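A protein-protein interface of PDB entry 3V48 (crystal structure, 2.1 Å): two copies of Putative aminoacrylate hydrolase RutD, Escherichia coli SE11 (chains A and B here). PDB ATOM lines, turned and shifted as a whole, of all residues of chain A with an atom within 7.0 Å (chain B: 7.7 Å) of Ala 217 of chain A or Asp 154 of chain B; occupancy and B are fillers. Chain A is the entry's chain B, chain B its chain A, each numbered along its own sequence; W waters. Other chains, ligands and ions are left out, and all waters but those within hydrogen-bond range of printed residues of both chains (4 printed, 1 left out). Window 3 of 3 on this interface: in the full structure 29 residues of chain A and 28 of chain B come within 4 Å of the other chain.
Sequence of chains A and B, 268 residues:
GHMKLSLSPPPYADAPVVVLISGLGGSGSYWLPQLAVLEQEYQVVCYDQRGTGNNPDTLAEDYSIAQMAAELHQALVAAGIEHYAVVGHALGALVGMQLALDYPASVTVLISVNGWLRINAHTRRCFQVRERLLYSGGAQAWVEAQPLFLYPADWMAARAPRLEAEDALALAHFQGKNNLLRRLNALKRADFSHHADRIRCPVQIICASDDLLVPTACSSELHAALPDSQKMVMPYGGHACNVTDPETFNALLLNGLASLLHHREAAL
Of the 9 printed residues of chain B, 4 touch a printed residue of chain A.
Hydrophobic or aromatic side chains of chain B within 4 Å of the printed part of chain A: Ala 153, Met 156 and Ala 157.
Along chain B the printed residues that touch a printed residue of chain A span positions 153 to 157.
Printed residues of chain A that touch a printed residue of chain B: Asn 120, His 122, Asp 211, Leu 212, Pro 215, Thr 216 and Ala 217.
Among the printed residues, 9 pairs touch across the chains.
The side-chain carboxylate (OD2) of Asp 154 of chain B sits at hydrogen-bond distance from the side-chain hydroxyl (OG1) of Thr 216 of chain A (2.6 Å).
The side-chain carboxylate (OD1) of Asp 154 of chain B lies within hydrogen-bond range of the backbone NH (N) of Ala 217 of chain A, at 3.0 Å.
No position is printed for both chains.
Of the 9 pairs that touch across the chains among the printed residues, none has its exchanged pair printed and touching as well.
Ala 157 of chain B touches Asn 120 of chain A.
Ala 153 of chain B touches His 122 of chain A.
CE1 of His 122 of chain A touches SD of Met 156 of chain B, at 3.6 Å.
Ala 153 of chain B touches Asp 211 of chain A (CB to O, 3.1 Å).
Ala 153 of chain B touches Leu 212 of chain A.
Pro 215 of chain A touches Asp 154 of chain B.
Pro 215 of chain A touches Ala 157 of chain B (CG to CB, 3.6 Å).
Ala 217 of chain A touches just one residue of chain B: Asp 154.
Of the printed residues of chain A, Asp 154 of chain B touches Pro 215 (3.3 Å), Thr 216 (2.6 Å) and Ala 217 (3.0 Å).
Printed residues of chain B within 4 Å of Asp 211 of chain A: Ala 153.
Printed residues of chain A within 4 Å of Ala 157 of chain B: Asn 120 (3.9 Å) and Pro 215 (3.6 Å).
Of the printed residues of chain B, Leu 212 of chain A touches Ala 153 (3.6 Å).
Printed residues of chain A within 4 Å of Met 156 of chain B: His 122.
The nearest residue of chain B that does not touch Ala 217 of chain A is Ala 157 of chain B (5.7 Å).
The nearest residue of chain A that does not touch Asp 154 of chain B is Ser 209 of chain A (4.3 Å).
The nearest printed residue of chain B that does not touch Asp 211 of chain A is Asp 154 of chain B (5.3 Å).
The side-chain carboxylate of Asp 211 of chain A sits at hydrogen-bond distance from the backbone NH of Val 214 of chain A.
NE2 of His 122 of chain A is in hydrogen-bond range of O of Leu 212 of chain A, 2.7 Å away.
The side-chain sulfur of Cys 218 of chain A lies close to the backbone carbonyl oxygen of Pro 215 of chain A.
The backbone NH (N) of His 122 of chain A sits at hydrogen-bond distance from the side-chain amide oxygen (OD1) of Asn 120 of chain A (2.9 Å).
Water W3 bridges OD2 of Asp 154 of chain B (2.6 Å) and O of Ser 209 of chain A (2.8 Å).
Water W1 bridges OD1 of Asn 120 of chain A (2.6 Å) and O of Ala 157 of chain B (3.0 Å).
Water W4 lies within hydrogen-bond range of the backbone carbonyl oxygen of Ser 209 of chain A, the backbone NH of Asp 154 of chain B and the backbone NH of Ala 153 of chain B.
Water W2 lies within hydrogen-bond range of the backbone carbonyl oxygen of Asp 211 of chain A and the backbone NH of Ala 153 of chain B.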
ATOM      1  N   GLY A 115     -23.327  -6.815  -0.252  1.00  0.00           N
ATOM      2  CA  GLY A 115     -24.023  -6.679  -1.512  1.00  0.00           C
ATOM      3  C   GLY A 115     -23.402  -7.572  -2.571  1.00  0.00           C
ATOM      4  O   GLY A 115     -22.579  -8.448  -2.277  1.00  0.00           O
ATOM      5  N   ASN A 120     -25.846 -14.433  -6.978  1.00  0.00           N
ATOM      6  CA  ASN A 120     -25.090 -15.688  -7.052  1.00  0.00           C
ATOM      7  C   ASN A 120     -26.048 -16.891  -7.071  1.00  0.00           C
ATOM      8  O   ASN A 120     -27.157 -16.832  -6.511  1.00  0.00           O
ATOM      9  CB  ASN A 120     -24.229 -15.738  -5.765  1.00  0.00           C
ATOM     10  CG  ASN A 120     -23.089 -16.693  -5.849  1.00  0.00           C
ATOM     11  OD1 ASN A 120     -23.210 -17.878  -5.529  1.00  0.00           O
ATOM     12  ND2 ASN A 120     -21.949 -16.181  -6.220  1.00  0.00           N
ATOM     13  N   HIS A 122     -25.621 -19.364  -5.133  1.00  0.00           N
ATOM     14  CA  HIS A 122     -25.774 -19.661  -3.716  1.00  0.00           C
ATOM     15  C   HIS A 122     -26.950 -18.899  -3.067  1.00  0.00           C
ATOM     16  O   HIS A 122     -27.774 -19.454  -2.366  1.00  0.00           O
ATOM     17  CB  HIS A 122     -24.491 -19.369  -2.944  1.00  0.00           C
ATOM     18  CG  HIS A 122     -24.629 -19.648  -1.473  1.00  0.00           C
ATOM     19  ND1 HIS A 122     -24.442 -20.891  -0.940  1.00  0.00           N
ATOM     20  CD2 HIS A 122     -25.034 -18.836  -0.428  1.00  0.00           C
ATOM     21  CE1 HIS A 122     -24.671 -20.844   0.380  1.00  0.00           C
ATOM     22  NE2 HIS A 122     -25.048 -19.598   0.692  1.00  0.00           N
ATOM     23  N   CYS A 207     -17.893  -6.586   3.935  1.00  0.00           N
ATOM     24  CA  CYS A 207     -18.519  -7.889   3.978  1.00  0.00           C
ATOM     25  C   CYS A 207     -18.027  -8.663   5.187  1.00  0.00           C
ATOM     26  O   CYS A 207     -17.069  -8.265   5.824  1.00  0.00           O
ATOM     27  CB  CYS A 207     -18.300  -8.649   2.672  1.00  0.00           C
ATOM     28  SG  CYS A 207     -16.593  -9.059   2.237  1.00  0.00           S
ATOM     29  N   ALA A 208     -18.702  -9.769   5.484  1.00  0.00           N
ATOM     30  CA  ALA A 208     -18.344 -10.659   6.584  1.00  0.00           C
ATOM     31  C   ALA A 208     -18.069 -12.084   6.054  1.00  0.00           C
ATOM     32  O   ALA A 208     -18.869 -12.673   5.292  1.00  0.00           O
ATOM     33  CB  ALA A 208     -19.431 -10.662   7.620  1.00  0.00           C
ATOM     34  N   SER A 209     -16.952 -12.642   6.469  1.00  0.00           N
ATOM     35  CA  SER A 209     -16.533 -13.953   5.983  1.00  0.00           C
ATOM     36  C   SER A 209     -17.547 -15.055   6.206  1.00  0.00           C
ATOM     37  O   SER A 209     -17.580 -16.029   5.465  1.00  0.00           O
ATOM     38  CB  SER A 209     -15.201 -14.344   6.600  1.00  0.00           C
ATOM     39  OG  SER A 209     -14.249 -13.383   6.299  1.00  0.00           O
ATOM     40  N   ASP A 210     -18.389 -14.861   7.207  1.00  0.00           N
ATOM     41  CA  ASP A 210     -19.336 -15.874   7.610  1.00  0.00           C
ATOM     42  C   ASP A 210     -20.772 -15.562   7.182  1.00  0.00           C
ATOM     43  O   ASP A 210     -21.690 -16.109   7.708  1.00  0.00           O
ATOM     44  CB  ASP A 210     -19.271 -16.101   9.112  1.00  0.00           C
ATOM     45  CG  ASP A 210     -19.607 -14.847   9.917  1.00  0.00           C
ATOM     46  OD1 ASP A 210     -19.672 -13.729   9.324  1.00  0.00           O
ATOM     47  OD2 ASP A 210     -19.744 -14.985  11.173  1.00  0.00           O
ATOM     48  N   ASP A 211     -20.926 -14.689   6.210  1.00  0.00           N
ATOM     49  CA  ASP A 211     -22.234 -14.378   5.649  1.00  0.00           C
ATOM     50  C   ASP A 211     -22.739 -15.649   4.979  1.00  0.00           C
ATOM     51  O   ASP A 211     -22.084 -16.166   4.096  1.00  0.00           O
ATOM     52  CB  ASP A 211     -22.119 -13.247   4.622  1.00  0.00           C
ATOM     53  CG  ASP A 211     -23.470 -12.801   4.087  1.00  0.00           C
ATOM     54  OD1 ASP A 211     -24.415 -13.613   4.096  1.00  0.00           O
ATOM     55  OD2 ASP A 211     -23.585 -11.635   3.680  1.00  0.00           O
ATOM     56  N   LEU A 212     -23.864 -16.174   5.464  1.00  0.00           N
ATOM     57  CA  LEU A 212     -24.430 -17.417   4.942  1.00  0.00           C
ATOM     58  C   LEU A 212     -25.256 -17.171   3.672  1.00  0.00           C
ATOM     59  O   LEU A 212     -25.367 -18.052   2.830  1.00  0.00           O
ATOM     60  CB  LEU A 212     -25.332 -18.098   5.997  1.00  0.00           C
ATOM     61  CG  LEU A 212     -25.672 -19.525   5.621  1.00  0.00           C
ATOM     62  CD1 LEU A 212     -24.482 -20.450   5.830  1.00  0.00           C
ATOM     63  CD2 LEU A 212     -26.910 -19.983   6.390  1.00  0.00           C
ATOM     64  N   VAL A 214     -25.096 -14.401   1.288  1.00  0.00           N
ATOM     65  CA  VAL A 214     -24.311 -13.851   0.201  1.00  0.00           C
ATOM     66  C   VAL A 214     -22.846 -14.204   0.444  1.00  0.00           C
ATOM     67  O   VAL A 214     -22.243 -13.718   1.391  1.00  0.00           O
ATOM     68  CB  VAL A 214     -24.484 -12.310   0.141  1.00  0.00           C
ATOM     69  CG1 VAL A 214     -23.767 -11.743  -1.091  1.00  0.00           C
ATOM     70  CG2 VAL A 214     -25.978 -11.996   0.132  1.00  0.00           C
ATOM     71  N   PRO A 215     -22.276 -15.062  -0.393  1.00  0.00           N
ATOM     72  CA  PRO A 215     -20.854 -15.345  -0.240  1.00  0.00           C
ATOM     73  C   PRO A 215     -19.989 -14.106  -0.529  1.00  0.00           C
ATOM     74  O   PRO A 215     -20.390 -13.255  -1.307  1.00  0.00           O
ATOM     75  CB  PRO A 215     -20.616 -16.465  -1.244  1.00  0.00           C
ATOM     76  CG  PRO A 215     -21.633 -16.260  -2.325  1.00  0.00           C
ATOM     77  CD  PRO A 215     -22.806 -15.547  -1.693  1.00  0.00           C
ATOM     78  N   THR A 216     -18.890 -13.939   0.202  1.00  0.00           N
ATOM     79  CA  THR A 216     -18.105 -12.696   0.113  1.00  0.00           C
ATOM     80  C   THR A 216     -17.439 -12.623  -1.240  1.00  0.00           C
ATOM     81  O   THR A 216     -17.001 -11.548  -1.648  1.00  0.00           O
ATOM     82  CB  THR A 216     -16.987 -12.568   1.182  1.00  0.00           C
ATOM     83  OG1 THR A 216     -16.031 -13.597   0.973  1.00  0.00           O
ATOM     84  CG2 THR A 216     -17.559 -12.630   2.605  1.00  0.00           C
ATOM     85  N   ALA A 217     -17.355 -13.753  -1.949  1.00  0.00           N
ATOM     86  CA  ALA A 217     -16.920 -13.698  -3.347  1.00  0.00           C
ATOM     87  C   ALA A 217     -17.763 -12.676  -4.122  1.00  0.00           C
ATOM     88  O   ALA A 217     -17.277 -12.106  -5.041  1.00  0.00           O
ATOM     89  CB  ALA A 217     -16.964 -15.041  -4.022  1.00  0.00           C
ATOM     90  N   CYS A 218     -19.006 -12.434  -3.729  1.00  0.00           N
ATOM     91  CA  CYS A 218     -19.810 -11.357  -4.369  1.00  0.00           C
ATOM     92  C   CYS A 218     -19.183  -9.986  -4.167  1.00  0.00           C
ATOM     93  O   CYS A 218     -19.086  -9.206  -5.103  1.00  0.00           O
ATOM     94  CB  CYS A 218     -21.239 -11.366  -3.854  1.00  0.00           C
ATOM     95  SG  CYS A 218     -22.126 -12.858  -4.375  1.00  0.00           S
ATOM     96  N   SER A 219     -18.682  -9.737  -2.961  1.00  0.00           N
ATOM     97  CA  SER A 219     -17.982  -8.474  -2.666  1.00  0.00           C
ATOM     98  C   SER A 219     -16.648  -8.385  -3.438  1.00  0.00           C
ATOM     99  O   SER A 219     -16.258  -7.325  -3.886  1.00  0.00           O
ATOM    100  CB  SER A 219     -17.768  -8.309  -1.155  1.00  0.00           C
ATOM    101  OG  SER A 219     -18.947  -7.822  -0.563  1.00  0.00           O
ATOM    102  N   SER A 220     -15.952  -9.503  -3.555  1.00  0.00           N
ATOM    103  CA  SER A 220     -14.727  -9.573  -4.375  1.00  0.00           C
ATOM    104  C   SER A 220     -15.012  -9.248  -5.827  1.00  0.00           C
ATOM    105  O   SER A 220     -14.306  -8.474  -6.424  1.00  0.00           O
ATOM    106  CB  SER A 220     -14.116 -10.946  -4.293  1.00  0.00           C
ATOM    107  OG  SER A 220     -13.690 -11.138  -2.961  1.00  0.00           O
ATOM    108  N   GLU A 221     -16.094  -9.815  -6.352  1.00  0.00           N
ATOM    109  CA  GLU A 221     -16.596  -9.484  -7.687  1.00  0.00           C
ATOM    110  C   GLU A 221     -16.891  -7.994  -7.860  1.00  0.00           C
ATOM    111  O   GLU A 221     -16.450  -7.363  -8.834  1.00  0.00           O
ATOM    112  CB  GLU A 221     -17.874 -10.263  -7.930  1.00  0.00           C
ATOM    113  CG  GLU A 221     -17.688 -11.483  -8.783  1.00  0.00           C
ATOM    114  CD  GLU A 221     -18.810 -12.461  -8.565  1.00  0.00           C
ATOM    115  OE1 GLU A 221     -19.984 -12.030  -8.607  1.00  0.00           O
ATOM    116  OE2 GLU A 221     -18.512 -13.643  -8.341  1.00  0.00           O
ATOM    117  N   LEU A 222     -17.620  -7.435  -6.900  1.00  0.00           N
ATOM    118  CA  LEU A 222     -17.936  -6.001  -6.885  1.00  0.00           C
ATOM    119  C   LEU A 222     -16.679  -5.169  -6.927  1.00  0.00           C
ATOM    120  O   LEU A 222     -16.553  -4.256  -7.744  1.00  0.00           O
ATOM    121  CB  LEU A 222     -18.693  -5.618  -5.625  1.00  0.00           C
ATOM    122  CG  LEU A 222     -20.162  -5.290  -5.627  1.00  0.00           C
ATOM    123  CD1 LEU A 222     -20.597  -4.973  -4.187  1.00  0.00           C
ATOM    124  CD2 LEU A 222     -20.461  -4.122  -6.519  1.00  0.00           C
ATOM    125  N   HIS A 223     -15.722  -5.532  -6.071  1.00  0.00           N
ATOM    126  CA  HIS A 223     -14.485  -4.808  -5.936  1.00  0.00           C
ATOM    127  C   HIS A 223     -13.672  -4.859  -7.231  1.00  0.00           C
ATOM    128  O   HIS A 223     -13.078  -3.874  -7.594  1.00  0.00           O
ATOM    129  CB  HIS A 223     -13.706  -5.361  -4.757  1.00  0.00           C
ATOM    130  CG  HIS A 223     -12.381  -4.689  -4.516  1.00  0.00           C
ATOM    131  ND1 HIS A 223     -12.260  -3.358  -4.393  1.00  0.00           N
ATOM    132  CD2 HIS A 223     -11.109  -5.216  -4.340  1.00  0.00           C
ATOM    133  CE1 HIS A 223     -10.978  -3.042  -4.147  1.00  0.00           C
ATOM    134  NE2 HIS A 223     -10.272  -4.171  -4.112  1.00  0.00           N
ATOM    135  N   LYS A 231     -12.222  -2.598  -0.266  1.00  0.00           N
ATOM    136  CA  LYS A 231     -12.954  -3.723   0.294  1.00  0.00           C
ATOM    137  C   LYS A 231     -12.443  -4.060   1.701  1.00  0.00           C
ATOM    138  O   LYS A 231     -11.249  -4.263   1.863  1.00  0.00           O
ATOM    139  CB  LYS A 231     -12.827  -4.940  -0.629  1.00  0.00           C
ATOM    140  CG  LYS A 231     -13.519  -6.187  -0.093  1.00  0.00           C
ATOM    141  CD  LYS A 231     -13.658  -7.257  -1.150  1.00  0.00           C
ATOM    142  CE  LYS A 231     -13.656  -8.632  -0.498  1.00  0.00           C
ATOM    143  NZ  LYS A 231     -12.282  -9.058  -0.179  1.00  0.00           N
ATOM    144  N   TYR B 151     -21.980 -26.175   5.426  1.00  0.00           N
ATOM    145  CA  TYR B 151     -20.804 -25.566   4.845  1.00  0.00           C
ATOM    146  C   TYR B 151     -20.840 -24.038   4.869  1.00  0.00           C
ATOM    147  O   TYR B 151     -21.915 -23.439   4.766  1.00  0.00           O
ATOM    148  CB  TYR B 151     -20.703 -25.969   3.390  1.00  0.00           C
ATOM    149  CG  TYR B 151     -20.784 -27.426   3.089  1.00  0.00           C
ATOM    150  CD1 TYR B 151     -20.021 -28.346   3.772  1.00  0.00           C
ATOM    151  CD2 TYR B 151     -21.546 -27.873   2.035  1.00  0.00           C
ATOM    152  CE1 TYR B 151     -20.034 -29.672   3.444  1.00  0.00           C
ATOM    153  CE2 TYR B 151     -21.575 -29.207   1.694  1.00  0.00           C
ATOM    154  CZ  TYR B 151     -20.821 -30.094   2.416  1.00  0.00           C
ATOM    155  OH  TYR B 151     -20.832 -31.412   2.082  1.00  0.00           O
ATOM    156  N   PRO B 152     -19.659 -23.395   4.980  1.00  0.00           N
ATOM    157  CA  PRO B 152     -19.641 -21.933   4.753  1.00  0.00           C
ATOM    158  C   PRO B 152     -20.110 -21.603   3.335  1.00  0.00           C
ATOM    159  O   PRO B 152     -19.872 -22.395   2.407  1.00  0.00           O
ATOM    160  CB  PRO B 152     -18.150 -21.563   4.921  1.00  0.00           C
ATOM    161  CG  PRO B 152     -17.584 -22.686   5.765  1.00  0.00           C
ATOM    162  CD  PRO B 152     -18.308 -23.909   5.274  1.00  0.00           C
ATOM    163  N   ALA B 153     -20.733 -20.435   3.202  1.00  0.00           N
ATOM    164  CA  ALA B 153     -21.223 -19.921   1.931  1.00  0.00           C
ATOM    165  C   ALA B 153     -20.129 -19.872   0.860  1.00  0.00           C
ATOM    166  O   ALA B 153     -20.342 -20.327  -0.236  1.00  0.00           O
ATOM    167  CB  ALA B 153     -21.899 -18.539   2.107  1.00  0.00           C
ATOM    168  N   ASP B 154     -18.972 -19.332   1.194  1.00  0.00           N
ATOM    169  CA  ASP B 154     -17.919 -19.201   0.185  1.00  0.00           C
ATOM    170  C   ASP B 154     -17.392 -20.542  -0.277  1.00  0.00           C
ATOM    171  O   ASP B 154     -17.062 -20.715  -1.453  1.00  0.00           O
ATOM    172  CB  ASP B 154     -16.753 -18.323   0.653  1.00  0.00           C
ATOM    173  CG  ASP B 154     -16.969 -16.840   0.324  1.00  0.00           C
ATOM    174  OD1 ASP B 154     -17.336 -16.508  -0.865  1.00  0.00           O
ATOM    175  OD2 ASP B 154     -16.768 -16.025   1.266  1.00  0.00           O
ATOM    176  N   TRP B 155     -17.372 -21.497   0.639  1.00  0.00           N
ATOM    177  CA  TRP B 155     -16.898 -22.829   0.326  1.00  0.00           C
ATOM    178  C   TRP B 155     -17.826 -23.447  -0.699  1.00  0.00           C
ATOM    179  O   TRP B 155     -17.404 -23.958  -1.725  1.00  0.00           O
ATOM    180  CB  TRP B 155     -16.760 -23.659   1.614  1.00  0.00           C
ATOM    181  CG  TRP B 155     -16.151 -24.998   1.377  1.00  0.00           C
ATOM    182  CD1 TRP B 155     -14.815 -25.348   1.500  1.00  0.00           C
ATOM    183  CD2 TRP B 155     -16.825 -26.202   0.894  1.00  0.00           C
ATOM    184  NE1 TRP B 155     -14.633 -26.652   1.156  1.00  0.00           N
ATOM    185  CE2 TRP B 155     -15.808 -27.226   0.806  1.00  0.00           C
ATOM    186  CE3 TRP B 155     -18.132 -26.524   0.575  1.00  0.00           C
ATOM    187  CZ2 TRP B 155     -16.105 -28.512   0.423  1.00  0.00           C
ATOM    188  CZ3 TRP B 155     -18.430 -27.820   0.194  1.00  0.00           C
ATOM    189  CH2 TRP B 155     -17.429 -28.793   0.103  1.00  0.00           C
ATOM    190  N   MET B 156     -19.115 -23.354  -0.426  1.00  0.00           N
ATOM    191  CA  MET B 156     -20.163 -23.849  -1.314  1.00  0.00           C
ATOM    192  C   MET B 156     -20.227 -23.120  -2.618  1.00  0.00           C
ATOM    193  O   MET B 156     -20.391 -23.730  -3.683  1.00  0.00           O
ATOM    194  CB  MET B 156     -21.483 -23.580  -0.624  1.00  0.00           C
ATOM    195  CG  MET B 156     -21.865 -24.741   0.260  1.00  0.00           C
ATOM    196  SD  MET B 156     -23.529 -24.197   1.162  1.00  0.00           S
ATOM    197  CE  MET B 156     -24.751 -24.631  -0.306  1.00  0.00           C
ATOM    198  N   ALA B 157     -20.116 -21.803  -2.548  1.00  0.00           N
ATOM    199  CA  ALA B 157     -20.286 -20.975  -3.749  1.00  0.00           C
ATOM    200  C   ALA B 157     -19.200 -21.228  -4.809  1.00  0.00           C
ATOM    201  O   ALA B 157     -19.428 -21.067  -6.006  1.00  0.00           O
ATOM    202  CB  ALA B 157     -20.374 -19.502  -3.389  1.00  0.00           C
ATOM    203  N   ALA B 158     -18.046 -21.684  -4.372  1.00  0.00           N
ATOM    204  CA  ALA B 158     -16.925 -21.898  -5.264  1.00  0.00           C
ATOM    205  C   ALA B 158     -16.996 -23.315  -5.849  1.00  0.00           C
ATOM    206  O   ALA B 158     -16.164 -23.684  -6.653  1.00  0.00           O
ATOM    207  CB  ALA B 158     -15.616 -21.681  -4.508  1.00  0.00           C
ATOM    208  N   ARG B 159     -17.986 -24.096  -5.414  1.00  0.00           N
ATOM    209  CA  ARG B 159     -18.041 -25.522  -5.704  1.00  0.00           C
ATOM    210  C   ARG B 159     -19.402 -25.980  -6.166  1.00  0.00           C
ATOM    211  O   ARG B 159     -19.845 -27.062  -5.764  1.00  0.00           O
ATOM    212  CB  ARG B 159     -17.658 -26.329  -4.457  1.00  0.00           C
ATOM    213  CG  ARG B 159     -16.237 -26.114  -4.006  1.00  0.00           C
ATOM    214  CD  ARG B 159     -15.982 -26.867  -2.724  1.00  0.00           C
ATOM    215  NE  ARG B 159     -14.584 -26.804  -2.352  1.00  0.00           N
ATOM    216  CZ  ARG B 159     -13.970 -25.716  -1.926  1.00  0.00           C
ATOM    217  NH1 ARG B 159     -14.605 -24.578  -1.767  1.00  0.00           N
ATOM    218  NH2 ARG B 159     -12.686 -25.775  -1.668  1.00  0.00           N
HETATM  219  O   HOH W   1     -22.222 -20.160  -6.358  1.00  0.00           O
HETATM  220  O   HOH W   2     -20.605 -18.367   5.204  1.00  0.00           O
HETATM  221  O   HOH W   3     -15.613 -16.256   3.537  1.00  0.00           O
HETATM  222  O   HOH W   4     -18.354 -18.185   3.799  1.00  0.00           O
